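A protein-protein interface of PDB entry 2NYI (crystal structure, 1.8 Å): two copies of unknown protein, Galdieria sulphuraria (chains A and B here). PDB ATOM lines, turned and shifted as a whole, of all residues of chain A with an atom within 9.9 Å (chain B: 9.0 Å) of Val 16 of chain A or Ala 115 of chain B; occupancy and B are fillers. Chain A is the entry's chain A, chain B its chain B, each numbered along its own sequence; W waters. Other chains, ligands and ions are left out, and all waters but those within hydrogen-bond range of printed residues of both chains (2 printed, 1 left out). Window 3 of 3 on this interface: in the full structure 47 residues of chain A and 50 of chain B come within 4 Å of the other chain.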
ATOM      1  N   SER A  13      -5.218 -13.126   5.880  1.00  0.00           N
ATOM      2  CA  SER A  13      -4.989 -12.041   4.925  1.00  0.00           C
ATOM      3  C   SER A  13      -6.104 -12.013   3.901  1.00  0.00           C
ATOM      4  O   SER A  13      -6.534 -13.061   3.392  1.00  0.00           O
ATOM      5  CB  SER A  13      -3.640 -12.203   4.216  1.00  0.00           C
ATOM      6  OG  SER A  13      -2.609 -12.294   5.181  1.00  0.00           O
ATOM      7  N   ASP A  14      -6.574 -10.812   3.596  1.00  0.00           N
ATOM      8  CA  ASP A  14      -7.682 -10.627   2.663  1.00  0.00           C
ATOM      9  C   ASP A  14      -7.316 -11.001   1.225  1.00  0.00           C
ATOM     10  O   ASP A  14      -6.180 -10.771   0.741  1.00  0.00           O
ATOM     11  CB  ASP A  14      -8.197  -9.190   2.722  1.00  0.00           C
ATOM     12  CG  ASP A  14      -9.540  -9.021   2.030  1.00  0.00           C
ATOM     13  OD1 ASP A  14     -10.371  -9.959   2.090  1.00  0.00           O
ATOM     14  OD2 ASP A  14      -9.772  -7.954   1.430  1.00  0.00           O
ATOM     15  N   ARG A  15      -8.303 -11.567   0.542  1.00  0.00           N
ATOM     16  CA  ARG A  15      -8.198 -11.858  -0.891  1.00  0.00           C
ATOM     17  C   ARG A  15      -9.618 -12.063  -1.406  1.00  0.00           C
ATOM     18  O   ARG A  15     -10.541 -12.286  -0.627  1.00  0.00           O
ATOM     19  CB  ARG A  15      -7.344 -13.105  -1.132  1.00  0.00           C
ATOM     20  CG  ARG A  15      -7.899 -14.380  -0.495  1.00  0.00           C
ATOM     21  CD  ARG A  15      -7.462 -15.629  -1.209  1.00  0.00           C
ATOM     22  NE  ARG A  15      -7.860 -16.846  -0.493  1.00  0.00           N
ATOM     23  CZ  ARG A  15      -9.016 -17.489  -0.637  1.00  0.00           C
ATOM     24  NH1 ARG A  15      -9.940 -17.057  -1.482  1.00  0.00           N
ATOM     25  NH2 ARG A  15      -9.238 -18.592   0.083  1.00  0.00           N
ATOM     26  N   VAL A  16      -9.792 -11.994  -2.726  1.00  0.00           N
ATOM     27  CA  VAL A  16     -11.094 -12.251  -3.312  1.00  0.00           C
ATOM     28  C   VAL A  16     -11.446 -13.721  -3.054  1.00  0.00           C
ATOM     29  O   VAL A  16     -10.569 -14.598  -3.116  1.00  0.00           O
ATOM     30  CB  VAL A  16     -11.103 -11.913  -4.827  1.00  0.00           C
ATOM     31  CG1 VAL A  16     -12.351 -12.462  -5.505  1.00  0.00           C
ATOM     32  CG2 VAL A  16     -11.023 -10.394  -5.023  1.00  0.00           C
ATOM     33  N   GLY A  17     -12.707 -13.977  -2.724  1.00  0.00           N
ATOM     34  CA  GLY A  17     -13.210 -15.348  -2.684  1.00  0.00           C
ATOM     35  C   GLY A  17     -13.205 -16.037  -1.340  1.00  0.00           C
ATOM     36  O   GLY A  17     -13.509 -17.221  -1.268  1.00  0.00           O
ATOM     37  N   ILE A  18     -12.828 -15.331  -0.279  1.00  0.00           N
ATOM     38  CA  ILE A  18     -12.815 -15.965   1.067  1.00  0.00           C
ATOM     39  C   ILE A  18     -14.224 -16.362   1.512  1.00  0.00           C
ATOM     40  O   ILE A  18     -14.476 -17.537   1.853  1.00  0.00           O
ATOM     41  CB  ILE A  18     -12.149 -15.071   2.148  1.00  0.00           C
ATOM     42  CG1 ILE A  18     -10.707 -14.777   1.773  1.00  0.00           C
ATOM     43  CG2 ILE A  18     -12.204 -15.782   3.584  1.00  0.00           C
ATOM     44  CD1 ILE A  18     -10.088 -13.634   2.613  1.00  0.00           C
ATOM     45  N   VAL A  19     -15.148 -15.396   1.478  1.00  0.00           N
ATOM     46  CA  VAL A  19     -16.518 -15.677   1.879  1.00  0.00           C
ATOM     47  C   VAL A  19     -17.076 -16.779   0.975  1.00  0.00           C
ATOM     48  O   VAL A  19     -17.806 -17.672   1.446  1.00  0.00           O
ATOM     49  CB  VAL A  19     -17.436 -14.453   1.863  1.00  0.00           C
ATOM     50  CG1 VAL A  19     -18.829 -14.859   2.366  1.00  0.00           C
ATOM     51  CG2 VAL A  19     -16.859 -13.306   2.776  1.00  0.00           C
ATOM     52  N   HIS A  20     -16.768 -16.716  -0.327  1.00  0.00           N
ATOM     53  CA  HIS A  20     -17.256 -17.783  -1.198  1.00  0.00           C
ATOM     54  C   HIS A  20     -16.732 -19.171  -0.809  1.00  0.00           C
ATOM     55  O   HIS A  20     -17.511 -20.140  -0.746  1.00  0.00           O
ATOM     56  CB  HIS A  20     -17.006 -17.502  -2.674  1.00  0.00           C
ATOM     57  CG  HIS A  20     -17.495 -18.614  -3.551  1.00  0.00           C
ATOM     58  ND1 HIS A  20     -16.638 -19.435  -4.244  1.00  0.00           N
ATOM     59  CD2 HIS A  20     -18.737 -19.121  -3.735  1.00  0.00           C
ATOM     60  CE1 HIS A  20     -17.337 -20.363  -4.878  1.00  0.00           C
ATOM     61  NE2 HIS A  20     -18.613 -20.195  -4.586  1.00  0.00           N
ATOM     62  N   ASP A  21     -15.428 -19.267  -0.573  1.00  0.00           N
ATOM     63  CA  ASP A  21     -14.797 -20.556  -0.229  1.00  0.00           C
ATOM     64  C   ASP A  21     -15.390 -21.109   1.050  1.00  0.00           C
ATOM     65  O   ASP A  21     -15.683 -22.305   1.146  1.00  0.00           O
ATOM     66  CB  ASP A  21     -13.276 -20.406  -0.113  1.00  0.00           C
ATOM     67  CG  ASP A  21     -12.601 -20.190  -1.463  1.00  0.00           C
ATOM     68  OD1 ASP A  21     -13.241 -20.397  -2.517  1.00  0.00           O
ATOM     69  OD2 ASP A  21     -11.422 -19.798  -1.465  1.00  0.00           O
ATOM     70  N   PHE A  22     -15.571 -20.216   2.027  1.00  0.00           N
ATOM     71  CA  PHE A  22     -16.208 -20.530   3.318  1.00  0.00           C
ATOM     72  C   PHE A  22     -17.624 -21.103   3.116  1.00  0.00           C
ATOM     73  O   PHE A  22     -17.975 -22.173   3.650  1.00  0.00           O
ATOM     74  CB  PHE A  22     -16.262 -19.238   4.162  1.00  0.00           C
ATOM     75  CG  PHE A  22     -16.885 -19.416   5.516  1.00  0.00           C
ATOM     76  CD1 PHE A  22     -16.092 -19.627   6.637  1.00  0.00           C
ATOM     77  CD2 PHE A  22     -18.269 -19.348   5.673  1.00  0.00           C
ATOM     78  CE1 PHE A  22     -16.684 -19.773   7.906  1.00  0.00           C
ATOM     79  CE2 PHE A  22     -18.859 -19.502   6.933  1.00  0.00           C
ATOM     80  CZ  PHE A  22     -18.056 -19.723   8.041  1.00  0.00           C
ATOM     81  N   SER A  23     -18.416 -20.385   2.319  1.00  0.00           N
ATOM     82  CA  SER A  23     -19.827 -20.710   2.075  1.00  0.00           C
ATOM     83  C   SER A  23     -19.957 -22.002   1.284  1.00  0.00           C
ATOM     84  O   SER A  23     -20.835 -22.832   1.559  1.00  0.00           O
ATOM     85  CB  SER A  23     -20.478 -19.563   1.294  1.00  0.00           C
ATOM     86  OG  SER A  23     -20.443 -18.387   2.086  1.00  0.00           O
ATOM     87  N   TRP A  24     -19.083 -22.169   0.294  1.00  0.00           N
ATOM     88  CA  TRP A  24     -19.054 -23.406  -0.476  1.00  0.00           C
ATOM     89  C   TRP A  24     -18.798 -24.601   0.452  1.00  0.00           C
ATOM     90  O   TRP A  24     -19.477 -25.639   0.360  1.00  0.00           O
ATOM     91  CB  TRP A  24     -18.004 -23.328  -1.589  1.00  0.00           C
ATOM     92  CG  TRP A  24     -18.049 -24.535  -2.443  1.00  0.00           C
ATOM     93  CD1 TRP A  24     -18.779 -24.704  -3.584  1.00  0.00           C
ATOM     94  CD2 TRP A  24     -17.389 -25.788  -2.191  1.00  0.00           C
ATOM     95  NE1 TRP A  24     -18.590 -25.983  -4.076  1.00  0.00           N
ATOM     96  CE2 TRP A  24     -17.739 -26.662  -3.246  1.00  0.00           C
ATOM     97  CE3 TRP A  24     -16.523 -26.248  -1.189  1.00  0.00           C
ATOM     98  CZ2 TRP A  24     -17.263 -27.978  -3.320  1.00  0.00           C
ATOM     99  CZ3 TRP A  24     -16.044 -27.564  -1.266  1.00  0.00           C
ATOM    100  CH2 TRP A  24     -16.419 -28.406  -2.326  1.00  0.00           C
ATOM    101  N   CYS A  40     -13.306  -6.349   6.934  1.00  0.00           N
ATOM    102  CA  CYS A  40     -12.040  -6.322   6.205  1.00  0.00           C
ATOM    103  C   CYS A  40     -11.448  -4.927   6.358  1.00  0.00           C
ATOM    104  O   CYS A  40     -12.159  -3.928   6.268  1.00  0.00           O
ATOM    105  CB  CYS A  40     -12.237  -6.609   4.712  1.00  0.00           C
ATOM    106  SG  CYS A  40     -12.321  -8.343   4.214  1.00  0.00           S
ATOM    107  N   GLY A  43      -5.839  -4.937   4.527  1.00  0.00           N
ATOM    108  CA  GLY A  43      -5.316  -6.206   4.002  1.00  0.00           C
ATOM    109  C   GLY A  43      -5.629  -7.445   4.836  1.00  0.00           C
ATOM    110  O   GLY A  43      -5.214  -8.560   4.486  1.00  0.00           O
ATOM    111  N   PHE A  45      -8.665  -9.852   6.924  1.00  0.00           N
ATOM    112  CA  PHE A  45     -10.034 -10.350   6.862  1.00  0.00           C
ATOM    113  C   PHE A  45     -10.381 -10.970   8.227  1.00  0.00           C
ATOM    114  O   PHE A  45      -9.592 -11.717   8.795  1.00  0.00           O
ATOM    115  CB  PHE A  45     -10.158 -11.405   5.722  1.00  0.00           C
ATOM    116  CG  PHE A  45     -11.465 -12.161   5.732  1.00  0.00           C
ATOM    117  CD1 PHE A  45     -12.461 -11.857   4.803  1.00  0.00           C
ATOM    118  CD2 PHE A  45     -11.694 -13.180   6.657  1.00  0.00           C
ATOM    119  CE1 PHE A  45     -13.686 -12.559   4.815  1.00  0.00           C
ATOM    120  CE2 PHE A  45     -12.915 -13.882   6.684  1.00  0.00           C
ATOM    121  CZ  PHE A  45     -13.906 -13.563   5.756  1.00  0.00           C
ATOM    122  N   ALA A  68     -10.891 -25.783   2.895  1.00  0.00           N
ATOM    123  CA  ALA A  68     -11.326 -24.723   1.975  1.00  0.00           C
ATOM    124  C   ALA A  68     -10.484 -23.446   2.098  1.00  0.00           C
ATOM    125  O   ALA A  68     -10.337 -22.703   1.123  1.00  0.00           O
ATOM    126  CB  ALA A  68     -12.802 -24.383   2.208  1.00  0.00           C
ATOM    127  N   LEU A  69      -9.937 -23.220   3.291  1.00  0.00           N
ATOM    128  CA  LEU A  69      -9.245 -21.961   3.647  1.00  0.00           C
ATOM    129  C   LEU A  69      -7.889 -22.263   4.279  1.00  0.00           C
ATOM    130  O   LEU A  69      -7.633 -21.909   5.437  1.00  0.00           O
ATOM    131  CB  LEU A  69     -10.107 -21.126   4.615  1.00  0.00           C
ATOM    132  CG  LEU A  69     -11.464 -20.641   4.092  1.00  0.00           C
ATOM    133  CD1 LEU A  69     -12.258 -19.959   5.209  1.00  0.00           C
ATOM    134  CD2 LEU A  69     -11.303 -19.728   2.886  1.00  0.00           C
ATOM    135  N   PHE A  72      -5.629 -19.963   6.922  1.00  0.00           N
ATOM    136  CA  PHE A  72      -6.497 -19.125   7.765  1.00  0.00           C
ATOM    137  C   PHE A  72      -6.537 -19.633   9.189  1.00  0.00           C
ATOM    138  O   PHE A  72      -6.376 -20.834   9.436  1.00  0.00           O
ATOM    139  CB  PHE A  72      -7.909 -19.003   7.175  1.00  0.00           C
ATOM    140  CG  PHE A  72      -7.984 -18.040   6.032  1.00  0.00           C
ATOM    141  CD1 PHE A  72      -8.466 -16.754   6.228  1.00  0.00           C
ATOM    142  CD2 PHE A  72      -7.520 -18.399   4.773  1.00  0.00           C
ATOM    143  CE1 PHE A  72      -8.510 -15.841   5.173  1.00  0.00           C
ATOM    144  CE2 PHE A  72      -7.563 -17.499   3.699  1.00  0.00           C
ATOM    145  CZ  PHE A  72      -8.039 -16.206   3.910  1.00  0.00           C
ATOM    146  N   VAL B 107     -26.118 -17.843   0.209  1.00  0.00           N
ATOM    147  CA  VAL B 107     -24.832 -17.150   0.398  1.00  0.00           C
ATOM    148  C   VAL B 107     -23.773 -17.641  -0.603  1.00  0.00           C
ATOM    149  O   VAL B 107     -23.102 -16.826  -1.268  1.00  0.00           O
ATOM    150  CB  VAL B 107     -24.351 -17.281   1.868  1.00  0.00           C
ATOM    151  CG1 VAL B 107     -22.968 -16.680   2.017  1.00  0.00           C
ATOM    152  CG2 VAL B 107     -25.351 -16.569   2.807  1.00  0.00           C
ATOM    153  N   GLU B 108     -23.643 -18.960  -0.746  1.00  0.00           N
ATOM    154  CA  GLU B 108     -22.722 -19.517  -1.765  1.00  0.00           C
ATOM    155  C   GLU B 108     -23.008 -19.001  -3.178  1.00  0.00           C
ATOM    156  O   GLU B 108     -22.063 -18.695  -3.920  1.00  0.00           O
ATOM    157  CB  GLU B 108     -22.696 -21.055  -1.752  1.00  0.00           C
ATOM    158  CG  GLU B 108     -21.548 -21.695  -2.580  1.00  0.00           C
ATOM    159  CD  GLU B 108     -21.796 -21.714  -4.106  1.00  0.00           C
ATOM    160  OE1 GLU B 108     -22.967 -21.706  -4.532  1.00  0.00           O
ATOM    161  OE2 GLU B 108     -20.807 -21.721  -4.873  1.00  0.00           O
ATOM    162  N   ALA B 109     -24.288 -18.922  -3.543  1.00  0.00           N
ATOM    163  CA  ALA B 109     -24.678 -18.499  -4.892  1.00  0.00           C
ATOM    164  C   ALA B 109     -24.335 -17.016  -5.150  1.00  0.00           C
ATOM    165  O   ALA B 109     -23.798 -16.664  -6.205  1.00  0.00           O
ATOM    166  CB  ALA B 109     -26.177 -18.765  -5.118  1.00  0.00           C
ATOM    167  N   VAL B 110     -24.631 -16.163  -4.169  1.00  0.00           N
ATOM    168  CA  VAL B 110     -24.392 -14.726  -4.287  1.00  0.00           C
ATOM    169  C   VAL B 110     -22.895 -14.455  -4.333  1.00  0.00           C
ATOM    170  O   VAL B 110     -22.403 -13.743  -5.226  1.00  0.00           O
ATOM    171  CB  VAL B 110     -25.064 -13.928  -3.122  1.00  0.00           C
ATOM    172  CG1 VAL B 110     -24.649 -12.465  -3.176  1.00  0.00           C
ATOM    173  CG2 VAL B 110     -26.621 -14.030  -3.192  1.00  0.00           C
ATOM    174  N   THR B 111     -22.171 -15.050  -3.381  1.00  0.00           N
ATOM    175  CA  THR B 111     -20.728 -14.887  -3.318  1.00  0.00           C
ATOM    176  C   THR B 111     -19.989 -15.548  -4.502  1.00  0.00           C
ATOM    177  O   THR B 111     -18.919 -15.075  -4.923  1.00  0.00           O
ATOM    178  CB  THR B 111     -20.158 -15.310  -1.941  1.00  0.00           C
ATOM    179  OG1 THR B 111     -20.410 -16.698  -1.706  1.00  0.00           O
ATOM    180  CG2 THR B 111     -20.819 -14.469  -0.796  1.00  0.00           C
ATOM    181  N   ALA B 112     -20.565 -16.614  -5.070  1.00  0.00           N
ATOM    182  CA  ALA B 112     -19.977 -17.197  -6.293  1.00  0.00           C
ATOM    183  C   ALA B 112     -19.940 -16.172  -7.423  1.00  0.00           C
ATOM    184  O   ALA B 112     -18.934 -16.045  -8.109  1.00  0.00           O
ATOM    185  CB  ALA B 112     -20.749 -18.457  -6.735  1.00  0.00           C
ATOM    186  N   VAL B 113     -21.034 -15.433  -7.593  1.00  0.00           N
ATOM    187  CA  VAL B 113     -21.126 -14.382  -8.617  1.00  0.00           C
ATOM    188  C   VAL B 113     -20.051 -13.317  -8.380  1.00  0.00           C
ATOM    189  O   VAL B 113     -19.273 -12.984  -9.278  1.00  0.00           O
ATOM    190  CB  VAL B 113     -22.559 -13.747  -8.645  1.00  0.00           C
ATOM    191  CG1 VAL B 113     -22.589 -12.487  -9.518  1.00  0.00           C
ATOM    192  CG2 VAL B 113     -23.586 -14.778  -9.171  1.00  0.00           C
ATOM    193  N   LEU B 114     -20.020 -12.797  -7.158  1.00  0.00           N
ATOM    194  CA  LEU B 114     -19.083 -11.734  -6.803  1.00  0.00           C
ATOM    195  C   LEU B 114     -17.628 -12.167  -7.003  1.00  0.00           C
ATOM    196  O   LEU B 114     -16.825 -11.413  -7.560  1.00  0.00           O
ATOM    197  CB  LEU B 114     -19.331 -11.272  -5.358  1.00  0.00           C
ATOM    198  CG  LEU B 114     -20.726 -10.699  -5.048  1.00  0.00           C
ATOM    199  CD1 LEU B 114     -20.868 -10.468  -3.554  1.00  0.00           C
ATOM    200  CD2 LEU B 114     -21.003  -9.409  -5.838  1.00  0.00           C
ATOM    201  N   ALA B 115     -17.284 -13.386  -6.587  1.00  0.00           N
ATOM    202  CA  ALA B 115     -15.903 -13.831  -6.715  1.00  0.00           C
ATOM    203  C   ALA B 115     -15.512 -14.095  -8.181  1.00  0.00           C
ATOM    204  O   ALA B 115     -14.411 -13.717  -8.621  1.00  0.00           O
ATOM    205  CB  ALA B 115     -15.615 -15.036  -5.810  1.00  0.00           C
ATOM    206  N   LYS B 116     -16.423 -14.709  -8.942  1.00  0.00           N
ATOM    207  CA  LYS B 116     -16.189 -14.946 -10.366  1.00  0.00           C
ATOM    208  C   LYS B 116     -15.943 -13.635 -11.119  1.00  0.00           C
ATOM    209  O   LYS B 116     -15.148 -13.595 -12.058  1.00  0.00           O
ATOM    210  CB  LYS B 116     -17.362 -15.711 -10.985  1.00  0.00           C
ATOM    211  CG  LYS B 116     -17.038 -16.305 -12.335  1.00  0.00           C
ATOM    212  CD  LYS B 116     -17.856 -17.552 -12.608  1.00  0.00           C
ATOM    213  CE  LYS B 116     -17.304 -18.282 -13.822  1.00  0.00           C
ATOM    214  NZ  LYS B 116     -17.981 -19.590 -14.047  1.00  0.00           N
ATOM    215  N   LYS B 117     -16.616 -12.568 -10.690  1.00  0.00           N
ATOM    216  CA  LYS B 117     -16.493 -11.240 -11.307  1.00  0.00           C
ATOM    217  C   LYS B 117     -15.346 -10.407 -10.722  1.00  0.00           C
ATOM    218  O   LYS B 117     -15.110  -9.277 -11.157  1.00  0.00           O
ATOM    219  CB  LYS B 117     -17.809 -10.470 -11.161  1.00  0.00           C
ATOM    220  CG  LYS B 117     -19.014 -11.060 -11.912  1.00  0.00           C
ATOM    221  CD  LYS B 117     -18.725 -11.305 -13.384  1.00  0.00           C
ATOM    222  CE  LYS B 117     -19.845 -12.116 -14.008  1.00  0.00           C
ATOM    223  NZ  LYS B 117     -19.689 -12.203 -15.473  1.00  0.00           N
ATOM    224  N   GLY B 118     -14.648 -10.963  -9.727  1.00  0.00           N
ATOM    225  CA  GLY B 118     -13.520 -10.290  -9.079  1.00  0.00           C
ATOM    226  C   GLY B 118     -13.868  -9.125  -8.162  1.00  0.00           C
ATOM    227  O   GLY B 118     -12.997  -8.284  -7.873  1.00  0.00           O
ATOM    228  N   ALA B 119     -15.115  -9.082  -7.675  1.00  0.00           N
ATOM    229  CA  ALA B 119     -15.528  -8.045  -6.737  1.00  0.00           C
ATOM    230  C   ALA B 119     -14.925  -8.276  -5.351  1.00  0.00           C
ATOM    231  O   ALA B 119     -14.794  -9.416  -4.904  1.00  0.00           O
ATOM    232  CB  ALA B 119     -17.056  -7.924  -6.681  1.00  0.00           C
ATOM    233  N   ASN B 120     -14.521  -7.191  -4.698  1.00  0.00           N
ATOM    234  CA  ASN B 120     -13.999  -7.253  -3.336  1.00  0.00           C
ATOM    235  C   ASN B 120     -15.167  -7.035  -2.386  1.00  0.00           C
ATOM    236  O   ASN B 120     -15.971  -6.135  -2.601  1.00  0.00           O
ATOM    237  CB  ASN B 120     -12.934  -6.168  -3.102  1.00  0.00           C
ATOM    238  CG  ASN B 120     -11.789  -6.234  -4.108  1.00  0.00           C
ATOM    239  OD1 ASN B 120     -10.902  -7.087  -4.009  1.00  0.00           O
ATOM    240  ND2 ASN B 120     -11.803  -5.322  -5.076  1.00  0.00           N
ATOM    241  N   ILE B 121     -15.292  -7.874  -1.367  1.00  0.00           N
ATOM    242  CA  ILE B 121     -16.313  -7.642  -0.322  1.00  0.00           C
ATOM    243  C   ILE B 121     -15.640  -6.853   0.795  1.00  0.00           C
ATOM    244  O   ILE B 121     -14.606  -7.272   1.331  1.00  0.00           O
ATOM    245  CB  ILE B 121     -16.947  -8.968   0.203  1.00  0.00           C
ATOM    246  CG1 ILE B 121     -17.485  -9.810  -0.975  1.00  0.00           C
ATOM    247  CG2 ILE B 121     -18.055  -8.676   1.224  1.00  0.00           C
ATOM    248  CD1 ILE B 121     -18.202 -11.142  -0.559  1.00  0.00           C
ATOM    249  N   VAL B 145     -19.709  -3.863  -1.500  1.00  0.00           N
ATOM    250  CA  VAL B 145     -18.765  -4.521  -2.406  1.00  0.00           C
ATOM    251  C   VAL B 145     -18.135  -3.456  -3.303  1.00  0.00           C
ATOM    252  O   VAL B 145     -18.694  -2.356  -3.446  1.00  0.00           O
ATOM    253  CB  VAL B 145     -19.444  -5.634  -3.276  1.00  0.00           C
ATOM    254  CG1 VAL B 145     -20.107  -6.686  -2.391  1.00  0.00           C
ATOM    255  CG2 VAL B 145     -20.447  -5.044  -4.244  1.00  0.00           C
ATOM    256  N   ALA B 146     -16.992  -3.771  -3.909  1.00  0.00           N
ATOM    257  CA  ALA B 146     -16.354  -2.823  -4.815  1.00  0.00           C
ATOM    258  C   ALA B 146     -15.879  -3.566  -6.036  1.00  0.00           C
ATOM    259  O   ALA B 146     -15.379  -4.693  -5.936  1.00  0.00           O
ATOM    260  CB  ALA B 146     -15.181  -2.109  -4.145  1.00  0.00           C
ATOM    261  N   PHE B 147     -16.077  -2.937  -7.191  1.00  0.00           N
ATOM    262  CA  PHE B 147     -15.610  -3.481  -8.474  1.00  0.00           C
ATOM    263  C   PHE B 147     -15.622  -2.353  -9.505  1.00  0.00           C
ATOM    264  O   PHE B 147     -16.241  -1.307  -9.263  1.00  0.00           O
ATOM    265  CB  PHE B 147     -16.444  -4.721  -8.928  1.00  0.00           C
ATOM    266  CG  PHE B 147     -17.936  -4.469  -9.052  1.00  0.00           C
ATOM    267  CD1 PHE B 147     -18.476  -3.901 -10.218  1.00  0.00           C
ATOM    268  CD2 PHE B 147     -18.811  -4.855  -8.034  1.00  0.00           C
ATOM    269  CE1 PHE B 147     -19.846  -3.677 -10.357  1.00  0.00           C
ATOM    270  CE2 PHE B 147     -20.184  -4.644  -8.150  1.00  0.00           C
ATOM    271  CZ  PHE B 147     -20.720  -4.049  -9.315  1.00  0.00           C
ATOM    272  N   LEU B 151     -18.367  -3.438 -15.041  1.00  0.00           N
ATOM    273  CA  LEU B 151     -18.865  -4.788 -14.749  1.00  0.00           C
ATOM    274  C   LEU B 151     -20.304  -4.777 -14.240  1.00  0.00           C
ATOM    275  O   LEU B 151     -20.906  -5.840 -14.084  1.00  0.00           O
ATOM    276  CB  LEU B 151     -17.989  -5.469 -13.681  1.00  0.00           C
ATOM    277  CG  LEU B 151     -16.564  -5.855 -14.085  1.00  0.00           C
ATOM    278  CD1 LEU B 151     -15.931  -6.751 -12.999  1.00  0.00           C
ATOM    279  CD2 LEU B 151     -16.536  -6.526 -15.460  1.00  0.00           C
ATOM    280  N   VAL B 155     -22.748  -8.112 -13.588  1.00  0.00           N
ATOM    281  CA  VAL B 155     -22.978  -8.517 -12.198  1.00  0.00           C
ATOM    282  C   VAL B 155     -24.491  -8.604 -11.930  1.00  0.00           C
ATOM    283  O   VAL B 155     -24.972  -9.631 -11.435  1.00  0.00           O
ATOM    284  CB  VAL B 155     -22.278  -7.567 -11.210  1.00  0.00           C
ATOM    285  CG1 VAL B 155     -22.710  -7.877  -9.767  1.00  0.00           C
ATOM    286  CG2 VAL B 155     -20.749  -7.674 -11.383  1.00  0.00           C
ATOM    287  N   LEU B 159     -26.583 -11.901 -10.912  1.00  0.00           N
ATOM    288  CA  LEU B 159     -27.374 -11.921  -9.673  1.00  0.00           C
ATOM    289  C   LEU B 159     -28.852 -12.229  -9.957  1.00  0.00           C
ATOM    290  O   LEU B 159     -29.520 -12.842  -9.138  1.00  0.00           O
ATOM    291  CB  LEU B 159     -27.224 -10.599  -8.899  1.00  0.00           C
ATOM    292  CG  LEU B 159     -25.830 -10.359  -8.299  1.00  0.00           C
ATOM    293  CD1 LEU B 159     -25.710  -8.945  -7.755  1.00  0.00           C
ATOM    294  CD2 LEU B 159     -25.527 -11.383  -7.213  1.00  0.00           C
HETATM  295  O   HOH W   1     -12.959 -10.127   1.463  1.00  0.00           O
HETATM  296  O   HOH W   2     -11.953  -6.597   0.634  1.00  0.00           O
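A ring nitrogen (NE2) of His 20 of chain A is in hydrogen-bond range of the side-chain carboxylate of Glu 108 of chain B, 2.7 Å away.
SG of Cys 40 of chain A sits at hydrogen-bond distance from OD1 of Asp 14 of chain A, 3.3 Å away.
O of Val 19 of chain A is in hydrogen-bond range of OG of Ser 23 of chain A (2.8 Å).
O of Val 107 of chain B is in hydrogen-bond range of OG1 of Thr 111 of chain B, 2.7 Å away.
The side-chain hydroxyl (OG1) of Thr 111 of chain B is in hydrogen-bond range of the backbone carbonyl oxygen (O) of Glu 108 of chain B.
N of Ala 119 of chain B sits at hydrogen-bond distance from O of Leu 114 of chain B (2.9 Å).
N of Ala 146 of chain B is in hydrogen-bond range of O of Asn 120 of chain B, at 2.9 Å.
Among the printed residues, pairs that only touch across the chains: Ser 23 of chain A with Val 107 of chain B, His 20 of chain A with Thr 111 of chain B, His 20 of chain A with Ala 112 of chain B, Val 16 of chain A with Asn 120 of chain B, Trp 24 of chain A with Glu 108 of chain B, Val 19 of chain A with Thr 111 of chain B, Ser 23 of chain A with Glu 108 of chain B, Cys 40 of chain A with Ile 121 of chain B, Val 16 of chain A with Ala 119 of chain B, Val 16 of chain A with Ala 115 of chain B and Gly 17 of chain A with Ala 115 of chain B.
Of chain B, only Ala 115 (3.9 Å), Ala 119 (3.9 Å) and Asn 120 (3.5 Å) come within 4 Å of Val 16 of chain A.
Of chain B, only Ala 115 (3.96 Å) comes within 4 Å of Gly 17 of chain A.
Of the printed residues of chain B, His 20 of chain A touches Glu 108 (2.7 Å), Thr 111 (3.4 Å) and Ala 112 (3.4 Å).
Printed residues of chain B within 4 Å of Ser 23 of chain A: Val 107 (3.0 Å) and Glu 108 (3.8 Å).
Ala 68 of chain A touches none of the printed residues of chain B.
Of the printed residues of chain A, Val 107 of chain B touches Ser 23.
Printed residues of chain A within 4 Å of Glu 108 of chain B: His 20 (2.7 Å), Ser 23 (3.8 Å) and Trp 24 (3.7 Å).
Ala 115 of chain B touches just these residues of chain A: Val 16 and Gly 17.
No residue of chain A comes within 4 Å of Gly 118 of chain B.
Printed residues of chain A within 4 Å of Ala 119 of chain B: Val 16 (3.9 Å).
Of the printed residues of chain A, Asn 120 of chain B touches Val 16.
The nearest residue of chain A that does not touch Ala 115 of chain B is His 20 of chain A (4.2 Å).
The nearest printed residue of chain A that does not touch Ala 112 of chain B is Val 19 of chain A (7.0 Å).
Of the 21 printed residues of chain B, 8 touch a printed residue of chain A.
Of the 18 printed residues of chain A, 7 touch a printed residue of chain B.
Printed residues of chain A that touch a printed residue of chain B: Val 16, Gly 17, Val 19, His 20, Ser 23, Trp 24 and Cys 40.
Along chain A the printed residues that touch a printed residue of chain B span positions 16 to 40.
No position is printed for both chains.
Of the 12 pairs that touch across the chains among the printed residues, none has its exchanged pair printed and touching as well.
Water W1 lies within hydrogen-bond range of OD1 of Asp 14 of chain A (2.7 Å), O of Ile 121 of chain B (3.3 Å) and SG of Cys 40 of chain A (3.3 Å).
Water W2 bridges OD2 of Asp 14 of chain A and O of Ile 121 of chain B.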
